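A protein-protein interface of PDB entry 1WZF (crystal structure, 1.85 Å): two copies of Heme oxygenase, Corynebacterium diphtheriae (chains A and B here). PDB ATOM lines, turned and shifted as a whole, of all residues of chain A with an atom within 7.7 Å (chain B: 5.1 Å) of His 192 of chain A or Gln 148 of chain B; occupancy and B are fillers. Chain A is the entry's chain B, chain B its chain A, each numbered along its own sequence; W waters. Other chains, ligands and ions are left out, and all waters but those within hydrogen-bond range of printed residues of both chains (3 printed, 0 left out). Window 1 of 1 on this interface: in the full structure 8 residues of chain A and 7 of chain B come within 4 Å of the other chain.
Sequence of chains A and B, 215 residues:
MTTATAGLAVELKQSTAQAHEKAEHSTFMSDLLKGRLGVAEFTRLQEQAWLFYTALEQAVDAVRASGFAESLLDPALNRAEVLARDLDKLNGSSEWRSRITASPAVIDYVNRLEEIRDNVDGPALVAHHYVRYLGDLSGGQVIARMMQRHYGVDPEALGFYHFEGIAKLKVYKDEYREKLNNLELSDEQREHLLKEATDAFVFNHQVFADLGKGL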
ATOM      1  N   ARG A 112      14.435 -26.944  -0.797  1.00  0.00           N
ATOM      2  CA  ARG A 112      15.069 -25.692  -0.347  1.00  0.00           C
ATOM      3  C   ARG A 112      14.660 -25.424   1.061  1.00  0.00           C
ATOM      4  O   ARG A 112      15.497 -25.007   1.859  1.00  0.00           O
ATOM      5  CB  ARG A 112      14.637 -24.489  -1.191  1.00  0.00           C
ATOM      6  CG  ARG A 112      15.223 -23.125  -0.779  1.00  0.00           C
ATOM      7  CD  ARG A 112      16.749 -23.089  -0.802  1.00  0.00           C
ATOM      8  NE  ARG A 112      17.277 -23.299  -2.152  1.00  0.00           N
ATOM      9  CZ  ARG A 112      17.339 -22.339  -3.076  1.00  0.00           C
ATOM     10  NH1 ARG A 112      17.819 -22.616  -4.283  1.00  0.00           N
ATOM     11  NH2 ARG A 112      16.949 -21.099  -2.787  1.00  0.00           N
ATOM     12  N   ILE A 116      17.158 -25.182   4.216  1.00  0.00           N
ATOM     13  CA  ILE A 116      17.107 -24.040   5.101  1.00  0.00           C
ATOM     14  C   ILE A 116      16.961 -24.478   6.566  1.00  0.00           C
ATOM     15  O   ILE A 116      17.669 -23.966   7.440  1.00  0.00           O
ATOM     16  CB  ILE A 116      16.003 -23.025   4.665  1.00  0.00           C
ATOM     17  CG1 ILE A 116      16.435 -22.253   3.392  1.00  0.00           C
ATOM     18  CG2 ILE A 116      15.540 -22.112   5.845  1.00  0.00           C
ATOM     19  CD1 ILE A 116      15.208 -21.421   2.792  1.00  0.00           C
ATOM     20  N   ASN A 119      20.333 -26.242   7.788  1.00  0.00           N
ATOM     21  CA  ASN A 119      21.450 -25.326   7.962  1.00  0.00           C
ATOM     22  C   ASN A 119      21.040 -24.239   8.987  1.00  0.00           C
ATOM     23  O   ASN A 119      21.829 -23.323   9.339  1.00  0.00           O
ATOM     24  CB  ASN A 119      21.810 -24.744   6.579  1.00  0.00           C
ATOM     25  CG  ASN A 119      23.091 -23.906   6.600  1.00  0.00           C
ATOM     26  OD1 ASN A 119      23.966 -24.140   7.454  1.00  0.00           O
ATOM     27  ND2 ASN A 119      23.232 -22.951   5.633  1.00  0.00           N
ATOM     28  N   ASP A 121      19.147 -21.713   8.565  1.00  0.00           N
ATOM     29  CA  ASP A 121      19.540 -20.499   7.840  1.00  0.00           C
ATOM     30  C   ASP A 121      18.520 -19.376   8.123  1.00  0.00           C
ATOM     31  O   ASP A 121      17.480 -19.278   7.486  1.00  0.00           O
ATOM     32  CB  ASP A 121      19.658 -20.877   6.357  1.00  0.00           C
ATOM     33  CG  ASP A 121      20.219 -19.750   5.472  1.00  0.00           C
ATOM     34  OD1 ASP A 121      20.339 -18.625   5.935  1.00  0.00           O
ATOM     35  OD2 ASP A 121      20.549 -20.015   4.293  1.00  0.00           O
ATOM     36  N   GLY A 122      18.813 -18.540   9.103  1.00  0.00           N
ATOM     37  CA  GLY A 122      17.846 -17.522   9.557  1.00  0.00           C
ATOM     38  C   GLY A 122      17.410 -16.553   8.439  1.00  0.00           C
ATOM     39  O   GLY A 122      16.202 -16.360   8.183  1.00  0.00           O
ATOM     40  N   PRO A 123      18.377 -15.838   7.841  1.00  0.00           N
ATOM     41  CA  PRO A 123      18.096 -14.935   6.699  1.00  0.00           C
ATOM     42  C   PRO A 123      17.260 -15.570   5.565  1.00  0.00           C
ATOM     43  O   PRO A 123      16.273 -14.963   5.057  1.00  0.00           O
ATOM     44  CB  PRO A 123      19.499 -14.591   6.197  1.00  0.00           C
ATOM     45  CG  PRO A 123      20.277 -14.505   7.550  1.00  0.00           C
ATOM     46  CD  PRO A 123      19.777 -15.737   8.297  1.00  0.00           C
ATOM     47  N   ALA A 124      17.638 -16.782   5.185  1.00  0.00           N
ATOM     48  CA  ALA A 124      16.913 -17.499   4.136  1.00  0.00           C
ATOM     49  C   ALA A 124      15.459 -17.766   4.559  1.00  0.00           C
ATOM     50  O   ALA A 124      14.512 -17.578   3.763  1.00  0.00           O
ATOM     51  CB  ALA A 124      17.593 -18.772   3.840  1.00  0.00           C
ATOM     52  N   LEU A 125      15.288 -18.177   5.813  1.00  0.00           N
ATOM     53  CA  LEU A 125      13.983 -18.510   6.291  1.00  0.00           C
ATOM     54  C   LEU A 125      13.098 -17.238   6.289  1.00  0.00           C
ATOM     55  O   LEU A 125      11.965 -17.277   5.831  1.00  0.00           O
ATOM     56  CB  LEU A 125      14.077 -19.168   7.685  1.00  0.00           C
ATOM     57  CG  LEU A 125      12.766 -19.626   8.339  1.00  0.00           C
ATOM     58  CD1 LEU A 125      12.036 -18.469   9.083  1.00  0.00           C
ATOM     59  CD2 LEU A 125      11.848 -20.379   7.312  1.00  0.00           C
ATOM     60  N   ALA A 127      13.274 -14.628   4.384  1.00  0.00           N
ATOM     61  CA  ALA A 127      12.909 -14.412   2.982  1.00  0.00           C
ATOM     62  C   ALA A 127      11.679 -15.213   2.594  1.00  0.00           C
ATOM     63  O   ALA A 127      10.681 -14.662   2.060  1.00  0.00           O
ATOM     64  CB  ALA A 127      14.066 -14.735   2.057  1.00  0.00           C
ATOM     65  N   HIS A 128      11.730 -16.516   2.901  1.00  0.00           N
ATOM     66  CA  HIS A 128      10.651 -17.440   2.499  1.00  0.00           C
ATOM     67  C   HIS A 128       9.338 -17.212   3.246  1.00  0.00           C
ATOM     68  O   HIS A 128       8.268 -17.392   2.688  1.00  0.00           O
ATOM     69  CB  HIS A 128      11.143 -18.876   2.627  1.00  0.00           C
ATOM     70  CG  HIS A 128      12.007 -19.293   1.491  1.00  0.00           C
ATOM     71  ND1 HIS A 128      11.501 -19.879   0.356  1.00  0.00           N
ATOM     72  CD2 HIS A 128      13.341 -19.174   1.299  1.00  0.00           C
ATOM     73  CE1 HIS A 128      12.492 -20.148  -0.480  1.00  0.00           C
ATOM     74  NE2 HIS A 128      13.619 -19.726   0.067  1.00  0.00           N
ATOM     75  N   SER A 186      24.208  -8.874   8.882  1.00  0.00           N
ATOM     76  CA  SER A 186      25.464  -8.489   8.257  1.00  0.00           C
ATOM     77  C   SER A 186      25.151  -8.220   6.784  1.00  0.00           C
ATOM     78  O   SER A 186      24.074  -8.658   6.267  1.00  0.00           O
ATOM     79  CB  SER A 186      26.496  -9.610   8.377  1.00  0.00           C
ATOM     80  OG  SER A 186      26.165 -10.682   7.526  1.00  0.00           O
ATOM     81  N   ASP A 187      26.080  -7.546   6.100  1.00  0.00           N
ATOM     82  CA  ASP A 187      25.903  -7.304   4.662  1.00  0.00           C
ATOM     83  C   ASP A 187      25.647  -8.603   3.923  1.00  0.00           C
ATOM     84  O   ASP A 187      24.725  -8.669   3.129  1.00  0.00           O
ATOM     85  CB  ASP A 187      27.097  -6.575   4.011  1.00  0.00           C
ATOM     86  CG  ASP A 187      27.257  -5.112   4.490  1.00  0.00           C
ATOM     87  OD1 ASP A 187      26.388  -4.571   5.219  1.00  0.00           O
ATOM     88  OD2 ASP A 187      28.280  -4.496   4.121  1.00  0.00           O
ATOM     89  N   GLU A 188      26.437  -9.644   4.201  1.00  0.00           N
ATOM     90  CA  GLU A 188      26.230 -10.942   3.544  1.00  0.00           C
ATOM     91  C   GLU A 188      24.862 -11.569   3.877  1.00  0.00           C
ATOM     92  O   GLU A 188      24.215 -12.164   3.021  1.00  0.00           O
ATOM     93  CB  GLU A 188      27.372 -11.907   3.894  1.00  0.00           C
ATOM     94  CG  GLU A 188      28.797 -11.398   3.558  1.00  0.00           C
ATOM     95  CD  GLU A 188      29.495 -10.594   4.681  1.00  0.00           C
ATOM     96  OE1 GLU A 188      30.741 -10.592   4.722  1.00  0.00           O
ATOM     97  OE2 GLU A 188      28.846  -9.935   5.499  1.00  0.00           O
ATOM     98  N   GLN A 189      24.431 -11.480   5.125  1.00  0.00           N
ATOM     99  CA  GLN A 189      23.096 -12.035   5.496  1.00  0.00           C
ATOM    100  C   GLN A 189      21.952 -11.342   4.749  1.00  0.00           C
ATOM    101  O   GLN A 189      20.993 -11.989   4.262  1.00  0.00           O
ATOM    102  CB  GLN A 189      22.854 -11.930   7.006  1.00  0.00           C
ATOM    103  CG  GLN A 189      23.660 -12.921   7.819  1.00  0.00           C
ATOM    104  CD  GLN A 189      23.467 -12.702   9.283  1.00  0.00           C
ATOM    105  OE1 GLN A 189      23.521 -11.544   9.772  1.00  0.00           O
ATOM    106  NE2 GLN A 189      23.206 -13.808  10.017  1.00  0.00           N
ATOM    107  N   ARG A 190      22.081 -10.033   4.602  1.00  0.00           N
ATOM    108  CA  ARG A 190      21.081  -9.217   3.920  1.00  0.00           C
ATOM    109  C   ARG A 190      21.068  -9.552   2.434  1.00  0.00           C
ATOM    110  O   ARG A 190      19.999  -9.742   1.869  1.00  0.00           O
ATOM    111  CB  ARG A 190      21.412  -7.727   4.146  1.00  0.00           C
ATOM    112  CG  ARG A 190      20.362  -6.703   3.629  1.00  0.00           C
ATOM    113  CD  ARG A 190      20.862  -5.313   4.020  1.00  0.00           C
ATOM    114  NE  ARG A 190      19.821  -4.300   3.973  1.00  0.00           N
ATOM    115  CZ  ARG A 190      19.478  -3.657   2.861  1.00  0.00           C
ATOM    116  NH1 ARG A 190      20.093  -3.976   1.712  1.00  0.00           N
ATOM    117  NH2 ARG A 190      18.525  -2.715   2.880  1.00  0.00           N
ATOM    118  N   GLU A 191      22.246  -9.648   1.798  1.00  0.00           N
ATOM    119  CA  GLU A 191      22.310 -10.157   0.404  1.00  0.00           C
ATOM    120  C   GLU A 191      21.687 -11.525   0.223  1.00  0.00           C
ATOM    121  O   GLU A 191      20.973 -11.785  -0.778  1.00  0.00           O
ATOM    122  CB  GLU A 191      23.772 -10.207  -0.084  1.00  0.00           C
ATOM    123  CG  GLU A 191      24.401  -8.804  -0.181  1.00  0.00           C
ATOM    124  CD  GLU A 191      25.916  -8.844  -0.364  1.00  0.00           C
ATOM    125  OE1 GLU A 191      26.478  -9.961  -0.544  1.00  0.00           O
ATOM    126  OE2 GLU A 191      26.511  -7.752  -0.341  1.00  0.00           O
ATOM    127  N   HIS A 192      21.984 -12.415   1.166  1.00  0.00           N
ATOM    128  CA  HIS A 192      21.384 -13.751   1.208  1.00  0.00           C
ATOM    129  C   HIS A 192      19.847 -13.726   1.312  1.00  0.00           C
ATOM    130  O   HIS A 192      19.146 -14.431   0.571  1.00  0.00           O
ATOM    131  CB  HIS A 192      22.071 -14.625   2.293  1.00  0.00           C
ATOM    132  CG  HIS A 192      21.618 -16.046   2.314  1.00  0.00           C
ATOM    133  ND1 HIS A 192      21.597 -16.830   1.182  1.00  0.00           N
ATOM    134  CD2 HIS A 192      21.119 -16.816   3.312  1.00  0.00           C
ATOM    135  CE1 HIS A 192      21.128 -18.026   1.483  1.00  0.00           C
ATOM    136  NE2 HIS A 192      20.847 -18.050   2.770  1.00  0.00           N
ATOM    137  N   LEU A 193      19.317 -12.914   2.219  1.00  0.00           N
ATOM    138  CA  LEU A 193      17.857 -12.742   2.384  1.00  0.00           C
ATOM    139  C   LEU A 193      17.220 -12.287   1.034  1.00  0.00           C
ATOM    140  O   LEU A 193      16.246 -12.919   0.512  1.00  0.00           O
ATOM    141  CB  LEU A 193      17.593 -11.750   3.568  1.00  0.00           C
ATOM    142  CG  LEU A 193      16.158 -11.672   4.089  1.00  0.00           C
ATOM    143  CD1 LEU A 193      16.174 -11.038   5.526  1.00  0.00           C
ATOM    144  CD2 LEU A 193      15.343 -10.817   3.071  1.00  0.00           C
ATOM    145  N   LEU A 194      17.864 -11.309   0.397  1.00  0.00           N
ATOM    146  CA  LEU A 194      17.386 -10.782  -0.894  1.00  0.00           C
ATOM    147  C   LEU A 194      17.450 -11.862  -1.982  1.00  0.00           C
ATOM    148  O   LEU A 194      16.483 -12.060  -2.692  1.00  0.00           O
ATOM    149  CB  LEU A 194      18.132  -9.504  -1.313  1.00  0.00           C
ATOM    150  CG  LEU A 194      17.875  -8.329  -0.359  1.00  0.00           C
ATOM    151  CD1 LEU A 194      18.910  -7.130  -0.530  1.00  0.00           C
ATOM    152  CD2 LEU A 194      16.441  -7.821  -0.443  1.00  0.00           C
ATOM    153  N   LYS A 195      18.528 -12.624  -2.015  1.00  0.00           N
ATOM    154  CA  LYS A 195      18.701 -13.679  -3.025  1.00  0.00           C
ATOM    155  C   LYS A 195      17.571 -14.711  -2.846  1.00  0.00           C
ATOM    156  O   LYS A 195      16.870 -15.055  -3.797  1.00  0.00           O
ATOM    157  CB  LYS A 195      20.119 -14.255  -2.886  1.00  0.00           C
ATOM    158  CG  LYS A 195      20.383 -15.779  -2.821  1.00  0.00           C
ATOM    159  CD  LYS A 195      19.874 -16.635  -3.993  1.00  0.00           C
ATOM    160  CE  LYS A 195      20.822 -17.773  -4.374  1.00  0.00           C
ATOM    161  NZ  LYS A 195      20.255 -19.175  -4.662  1.00  0.00           N
ATOM    162  N   GLU A 196      17.402 -15.170  -1.603  1.00  0.00           N
ATOM    163  CA  GLU A 196      16.362 -16.139  -1.250  1.00  0.00           C
ATOM    164  C   GLU A 196      14.945 -15.687  -1.517  1.00  0.00           C
ATOM    165  O   GLU A 196      14.123 -16.529  -1.902  1.00  0.00           O
ATOM    166  CB  GLU A 196      16.514 -16.612   0.212  1.00  0.00           C
ATOM    167  CG  GLU A 196      17.741 -17.593   0.381  1.00  0.00           C
ATOM    168  CD  GLU A 196      17.495 -18.995  -0.192  1.00  0.00           C
ATOM    169  OE1 GLU A 196      16.334 -19.435  -0.444  1.00  0.00           O
ATOM    170  OE2 GLU A 196      18.493 -19.713  -0.328  1.00  0.00           O
ATOM    171  N   ALA A 197      14.668 -14.383  -1.354  1.00  0.00           N
ATOM    172  CA  ALA A 197      13.312 -13.850  -1.601  1.00  0.00           C
ATOM    173  C   ALA A 197      12.948 -13.934  -3.080  1.00  0.00           C
ATOM    174  O   ALA A 197      11.850 -14.386  -3.424  1.00  0.00           O
ATOM    175  CB  ALA A 197      13.168 -12.436  -1.052  1.00  0.00           C
ATOM    176  N   THR A 198      13.903 -13.572  -3.952  1.00  0.00           N
ATOM    177  CA  THR A 198      13.724 -13.821  -5.377  1.00  0.00           C
ATOM    178  C   THR A 198      13.477 -15.293  -5.653  1.00  0.00           C
ATOM    179  O   THR A 198      12.477 -15.623  -6.328  1.00  0.00           O
ATOM    180  CB  THR A 198      14.817 -13.165  -6.266  1.00  0.00           C
ATOM    181  OG1 THR A 198      14.523 -11.770  -6.358  1.00  0.00           O
ATOM    182  CG2 THR A 198      14.818 -13.720  -7.687  1.00  0.00           C
ATOM    183  N   ASP A 199      14.353 -16.174  -5.151  1.00  0.00           N
ATOM    184  CA  ASP A 199      14.122 -17.625  -5.296  1.00  0.00           C
ATOM    185  C   ASP A 199      12.746 -18.102  -4.860  1.00  0.00           C
ATOM    186  O   ASP A 199      12.175 -18.958  -5.526  1.00  0.00           O
ATOM    187  CB  ASP A 199      15.169 -18.446  -4.571  1.00  0.00           C
ATOM    188  CG  ASP A 199      16.531 -18.397  -5.232  1.00  0.00           C
ATOM    189  OD1 ASP A 199      16.687 -17.814  -6.354  1.00  0.00           O
ATOM    190  OD2 ASP A 199      17.435 -18.985  -4.601  1.00  0.00           O
ATOM    191  N   ALA B 144      34.306 -17.241  -0.692  1.00  0.00           N
ATOM    192  CA  ALA B 144      33.677 -17.113   0.634  1.00  0.00           C
ATOM    193  C   ALA B 144      32.434 -16.179   0.643  1.00  0.00           C
ATOM    194  O   ALA B 144      31.399 -16.489   1.272  1.00  0.00           O
ATOM    195  CB  ALA B 144      34.732 -16.594   1.650  1.00  0.00           C
ATOM    196  N   ARG B 145      32.572 -14.989   0.032  1.00  0.00           N
ATOM    197  CA  ARG B 145      31.462 -14.046  -0.089  1.00  0.00           C
ATOM    198  C   ARG B 145      30.275 -14.680  -0.803  1.00  0.00           C
ATOM    199  O   ARG B 145      29.120 -14.515  -0.373  1.00  0.00           O
ATOM    200  CB  ARG B 145      31.894 -12.769  -0.806  1.00  0.00           C
ATOM    201  CG  ARG B 145      30.828 -11.646  -0.909  1.00  0.00           C
ATOM    202  CD  ARG B 145      30.070 -11.381   0.408  1.00  0.00           C
ATOM    203  NE  ARG B 145      29.316 -10.116   0.442  1.00  0.00           N
ATOM    204  CZ  ARG B 145      29.821  -8.983   0.926  1.00  0.00           C
ATOM    205  NH1 ARG B 145      31.064  -8.978   1.420  1.00  0.00           N
ATOM    206  NH2 ARG B 145      29.087  -7.868   0.927  1.00  0.00           N
ATOM    207  N   MET B 146      30.540 -15.380  -1.900  1.00  0.00           N
ATOM    208  CA  MET B 146      29.478 -16.075  -2.631  1.00  0.00           C
ATOM    209  C   MET B 146      28.781 -17.194  -1.805  1.00  0.00           C
ATOM    210  O   MET B 146      27.595 -17.435  -1.949  1.00  0.00           O
ATOM    211  CB  MET B 146      30.004 -16.615  -3.965  1.00  0.00           C
ATOM    212  CG  MET B 146      30.337 -15.497  -4.997  1.00  0.00           C
ATOM    213  SD  MET B 146      28.977 -14.312  -5.197  1.00  0.00           S
ATOM    214  CE  MET B 146      29.261 -13.143  -3.924  1.00  0.00           C
ATOM    215  N   MET B 147      29.536 -17.869  -0.945  1.00  0.00           N
ATOM    216  CA  MET B 147      28.974 -18.966  -0.154  1.00  0.00           C
ATOM    217  C   MET B 147      28.080 -18.393   0.920  1.00  0.00           C
ATOM    218  O   MET B 147      27.038 -18.960   1.265  1.00  0.00           O
ATOM    219  CB  MET B 147      30.065 -19.874   0.408  1.00  0.00           C
ATOM    220  CG  MET B 147      31.004 -20.513  -0.529  1.00  0.00           C
ATOM    221  SD  MET B 147      30.137 -21.510  -1.778  1.00  0.00           S
ATOM    222  CE  MET B 147      29.847 -20.344  -3.138  1.00  0.00           C
ATOM    223  N   GLN B 148      28.423 -17.237   1.468  1.00  0.00           N
ATOM    224  CA  GLN B 148      27.427 -16.617   2.368  1.00  0.00           C
ATOM    225  C   GLN B 148      26.216 -16.041   1.633  1.00  0.00           C
ATOM    226  O   GLN B 148      25.066 -16.202   2.112  1.00  0.00           O
ATOM    227  CB  GLN B 148      28.062 -15.506   3.217  1.00  0.00           C
ATOM    228  CG  GLN B 148      29.287 -15.908   3.981  1.00  0.00           C
ATOM    229  CD  GLN B 148      29.681 -14.821   4.935  1.00  0.00           C
ATOM    230  OE1 GLN B 148      30.803 -14.283   4.871  1.00  0.00           O
ATOM    231  NE2 GLN B 148      28.758 -14.467   5.810  1.00  0.00           N
ATOM    232  N   ARG B 149      26.458 -15.330   0.510  1.00  0.00           N
ATOM    233  CA  ARG B 149      25.362 -14.701  -0.260  1.00  0.00           C
ATOM    234  C   ARG B 149      24.336 -15.705  -0.705  1.00  0.00           C
ATOM    235  O   ARG B 149      23.146 -15.493  -0.579  1.00  0.00           O
ATOM    236  CB  ARG B 149      25.878 -13.935  -1.499  1.00  0.00           C
ATOM    237  CG  ARG B 149      24.733 -13.337  -2.373  1.00  0.00           C
ATOM    238  CD  ARG B 149      25.326 -12.474  -3.525  1.00  0.00           C
ATOM    239  NE  ARG B 149      26.201 -11.408  -2.994  1.00  0.00           N
ATOM    240  CZ  ARG B 149      26.931 -10.573  -3.745  1.00  0.00           C
ATOM    241  NH1 ARG B 149      26.913 -10.669  -5.066  1.00  0.00           N
ATOM    242  NH2 ARG B 149      27.680  -9.644  -3.172  1.00  0.00           N
ATOM    243  N   HIS B 150      24.819 -16.811  -1.254  1.00  0.00           N
ATOM    244  CA  HIS B 150      23.944 -17.745  -1.925  1.00  0.00           C
ATOM    245  C   HIS B 150      23.448 -18.850  -1.037  1.00  0.00           C
ATOM    246  O   HIS B 150      22.331 -19.292  -1.233  1.00  0.00           O
ATOM    247  CB  HIS B 150      24.665 -18.422  -3.103  1.00  0.00           C
ATOM    248  CG  HIS B 150      24.892 -17.510  -4.265  1.00  0.00           C
ATOM    249  ND1 HIS B 150      23.942 -16.600  -4.677  1.00  0.00           N
ATOM    250  CD2 HIS B 150      25.944 -17.376  -5.107  1.00  0.00           C
ATOM    251  CE1 HIS B 150      24.406 -15.933  -5.720  1.00  0.00           C
ATOM    252  NE2 HIS B 150      25.620 -16.374  -5.989  1.00  0.00           N
ATOM    253  N   TYR B 151      24.309 -19.347  -0.151  1.00  0.00           N
ATOM    254  CA  TYR B 151      24.014 -20.549   0.636  1.00  0.00           C
ATOM    255  C   TYR B 151      23.989 -20.310   2.154  1.00  0.00           C
ATOM    256  O   TYR B 151      23.856 -21.262   2.930  1.00  0.00           O
ATOM    257  CB  TYR B 151      24.977 -21.657   0.253  1.00  0.00           C
ATOM    258  CG  TYR B 151      25.063 -21.814  -1.271  1.00  0.00           C
ATOM    259  CD1 TYR B 151      26.304 -21.719  -1.947  1.00  0.00           C
ATOM    260  CD2 TYR B 151      23.911 -22.002  -2.036  1.00  0.00           C
ATOM    261  CE1 TYR B 151      26.387 -21.843  -3.332  1.00  0.00           C
ATOM    262  CE2 TYR B 151      24.000 -22.140  -3.460  1.00  0.00           C
ATOM    263  CZ  TYR B 151      25.235 -22.053  -4.070  1.00  0.00           C
ATOM    264  OH  TYR B 151      25.311 -22.157  -5.435  1.00  0.00           O
ATOM    265  N   GLY B 152      24.120 -19.062   2.584  1.00  0.00           N
ATOM    266  CA  GLY B 152      23.948 -18.769   4.009  1.00  0.00           C
ATOM    267  C   GLY B 152      24.974 -19.454   4.908  1.00  0.00           C
ATOM    268  O   GLY B 152      24.703 -19.716   6.077  1.00  0.00           O
ATOM    269  N   VAL B 153      26.165 -19.729   4.378  1.00  0.00           N
ATOM    270  CA  VAL B 153      27.191 -20.484   5.129  1.00  0.00           C
ATOM    271  C   VAL B 153      27.726 -19.619   6.258  1.00  0.00           C
ATOM    272  O   VAL B 153      28.096 -18.464   6.047  1.00  0.00           O
ATOM    273  CB  VAL B 153      28.355 -20.951   4.221  1.00  0.00           C
ATOM    274  CG1 VAL B 153      29.502 -21.569   5.045  1.00  0.00           C
ATOM    275  CG2 VAL B 153      27.842 -21.990   3.201  1.00  0.00           C
ATOM    276  N   PRO B 155      30.031 -17.775   8.628  1.00  0.00           N
ATOM    277  CA  PRO B 155      31.386 -17.270   8.352  1.00  0.00           C
ATOM    278  C   PRO B 155      32.415 -18.107   9.133  1.00  0.00           C
ATOM    279  O   PRO B 155      33.542 -18.238   8.729  1.00  0.00           O
ATOM    280  CB  PRO B 155      31.358 -15.823   8.911  1.00  0.00           C
ATOM    281  CG  PRO B 155      29.969 -15.488   9.117  1.00  0.00           C
ATOM    282  CD  PRO B 155      29.163 -16.737   9.242  1.00  0.00           C
ATOM    283  N   LEU B 158      33.934 -20.902   7.192  1.00  0.00           N
ATOM    284  CA  LEU B 158      34.761 -20.483   6.052  1.00  0.00           C
ATOM    285  C   LEU B 158      36.174 -20.145   6.514  1.00  0.00           C
ATOM    286  O   LEU B 158      36.850 -19.268   5.918  1.00  0.00           O
ATOM    287  CB  LEU B 158      34.121 -19.274   5.332  1.00  0.00           C
ATOM    288  CG  LEU B 158      32.684 -19.564   4.843  1.00  0.00           C
ATOM    289  CD1 LEU B 158      31.981 -18.221   4.492  1.00  0.00           C
ATOM    290  CD2 LEU B 158      32.721 -20.482   3.605  1.00  0.00           C
HETATM  291  O   HOH W   1      31.589 -12.092   7.188  1.00  0.00           O
HETATM  292  O   HOH W   2      20.364 -20.499  -2.158  1.00  0.00           O
HETATM  293  O   HOH W   3      27.929 -12.770   7.951  1.00  0.00           O
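The guanidinium group (NH1) of Arg 145 of chain B lies within salt-bridge range of the side-chain carboxylate (OE1) of Glu 188 of chain A (3.7 Å).
OE2 of Glu 191 of chain A lies within salt-bridge range of NH2 of Arg 145 of chain B (2.9 Å).
OE1 of Glu 191 of chain A is in salt-bridge range of NE of Arg 149 of chain B, at 2.9 Å.
A ring nitrogen (ND1) of His 192 of chain A lies within hydrogen-bond range of the backbone carbonyl oxygen of Arg 149 of chain B, at 2.7 Å.
The backbone carbonyl oxygen (O) of Tyr 151 of chain B sits at hydrogen-bond distance from the side-chain amide nitrogen (ND2) of Asn 119 of chain A.
N of Gly 152 of chain B sits close to NE2 of His 192 of chain A (3.4 Å).
The guanidinium group of Arg 112 of chain A lies within salt-bridge range of the side-chain carboxylate of Glu 196 of chain A, 2.9 Å away.
OD2 of Asp 121 of chain A lies within hydrogen-bond range of NE2 of His 192 of chain A.
A ring nitrogen (NE2) of His 128 of chain A is in hydrogen-bond range of the side-chain carboxylate (OE1) of Glu 196 of chain A, 2.8 Å away.
OE2 of Glu 188 of chain A sits at hydrogen-bond distance from OG of Ser 186 of chain A (3.4 Å).
NZ of Lys 195 of chain A lies within salt-bridge range of OD2 of Asp 199 of chain A, 2.8 Å away.
Among the printed residues, merely in contact across the chains: His 192 of chain A with His 150 of chain B (3.2 Å), Lys 195 of chain A with His 150 of chain B (3.3 Å), His 192 of chain A with Gln 148 of chain B (3.4 Å), Glu 188 of chain A with Gln 148 of chain B (3.5 Å), Lys 195 of chain A with Arg 149 of chain B (3.6 Å), Asn 119 of chain A with Gly 152 of chain B (3.6 Å), Asp 121 of chain A with Gly 152 of chain B (3.6 Å), His 192 of chain A with Tyr 151 of chain B (3.7 Å), Asp 121 of chain A with Tyr 151 of chain B (3.8 Å), Asp 187 of chain A with Arg 145 of chain B (3.9 Å) and Glu 196 of chain A with His 150 of chain B (3.97 Å).
Ile 116 of chain A touches none of the printed residues of chain B.
Printed residues of chain B within 4 Å of Glu 191 of chain A: Arg 145 and Arg 149.
His 192 of chain A touches just these residues of chain B: Gln 148, Arg 149, His 150, Tyr 151 and Gly 152.
Of the printed residues of chain A, Arg 149 of chain B touches Glu 191 (2.9 Å), His 192 (2.7 Å) and Lys 195 (3.6 Å).
Printed residues of chain A within 4 Å of Gly 152 of chain B: Asn 119 (3.6 Å), Asp 121 (3.6 Å) and His 192 (3.4 Å).
Val 153 of chain B touches none of the printed residues of chain A.
The nearest printed residue of chain B that does not touch His 192 of chain A is Val 153 of chain B (5.8 Å).
The nearest residue of chain A that does not touch Gln 148 of chain B is Ser 186 of chain A (4.9 Å).
Printed residues of chain A that touch a printed residue of chain B: Asn 119, Asp 121, Asp 187, Glu 188, Glu 191, His 192, Lys 195 and Glu 196.
Hydrophobic or aromatic side chains of chain A that line the printed part of chain B: His 192.
Printed residues of chain B that touch a printed residue of chain A: Arg 145, Gln 148, Arg 149, His 150, Tyr 151 and Gly 152.
Among the printed residues, Asp or Glu carboxylates within 4 Å of a Lys or Arg side-chain nitrogen of the other chain: Glu 188 of chain A with Arg 145 of chain B, Glu 191 of chain A with Arg 145 of chain B and Glu 191 of chain A with Arg 149 of chain B.
No position is printed for both chains.
Of the 17 pairs that touch across the chains among the printed residues, none has its exchanged pair printed and touching as well.
Water W2 lies within hydrogen-bond range of O of His 150 of chain B, OE2 of Glu 196 of chain A and NZ of Lys 195 of chain A.
Water W3 bridges OG of Ser 186 of chain A and NE2 of Gln 148 of chain B.
Water W1 lies within hydrogen-bond range of OE1 of Glu 188 of chain A (3.0 Å) and OE1 of Gln 148 of chain B (3.3 Å).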
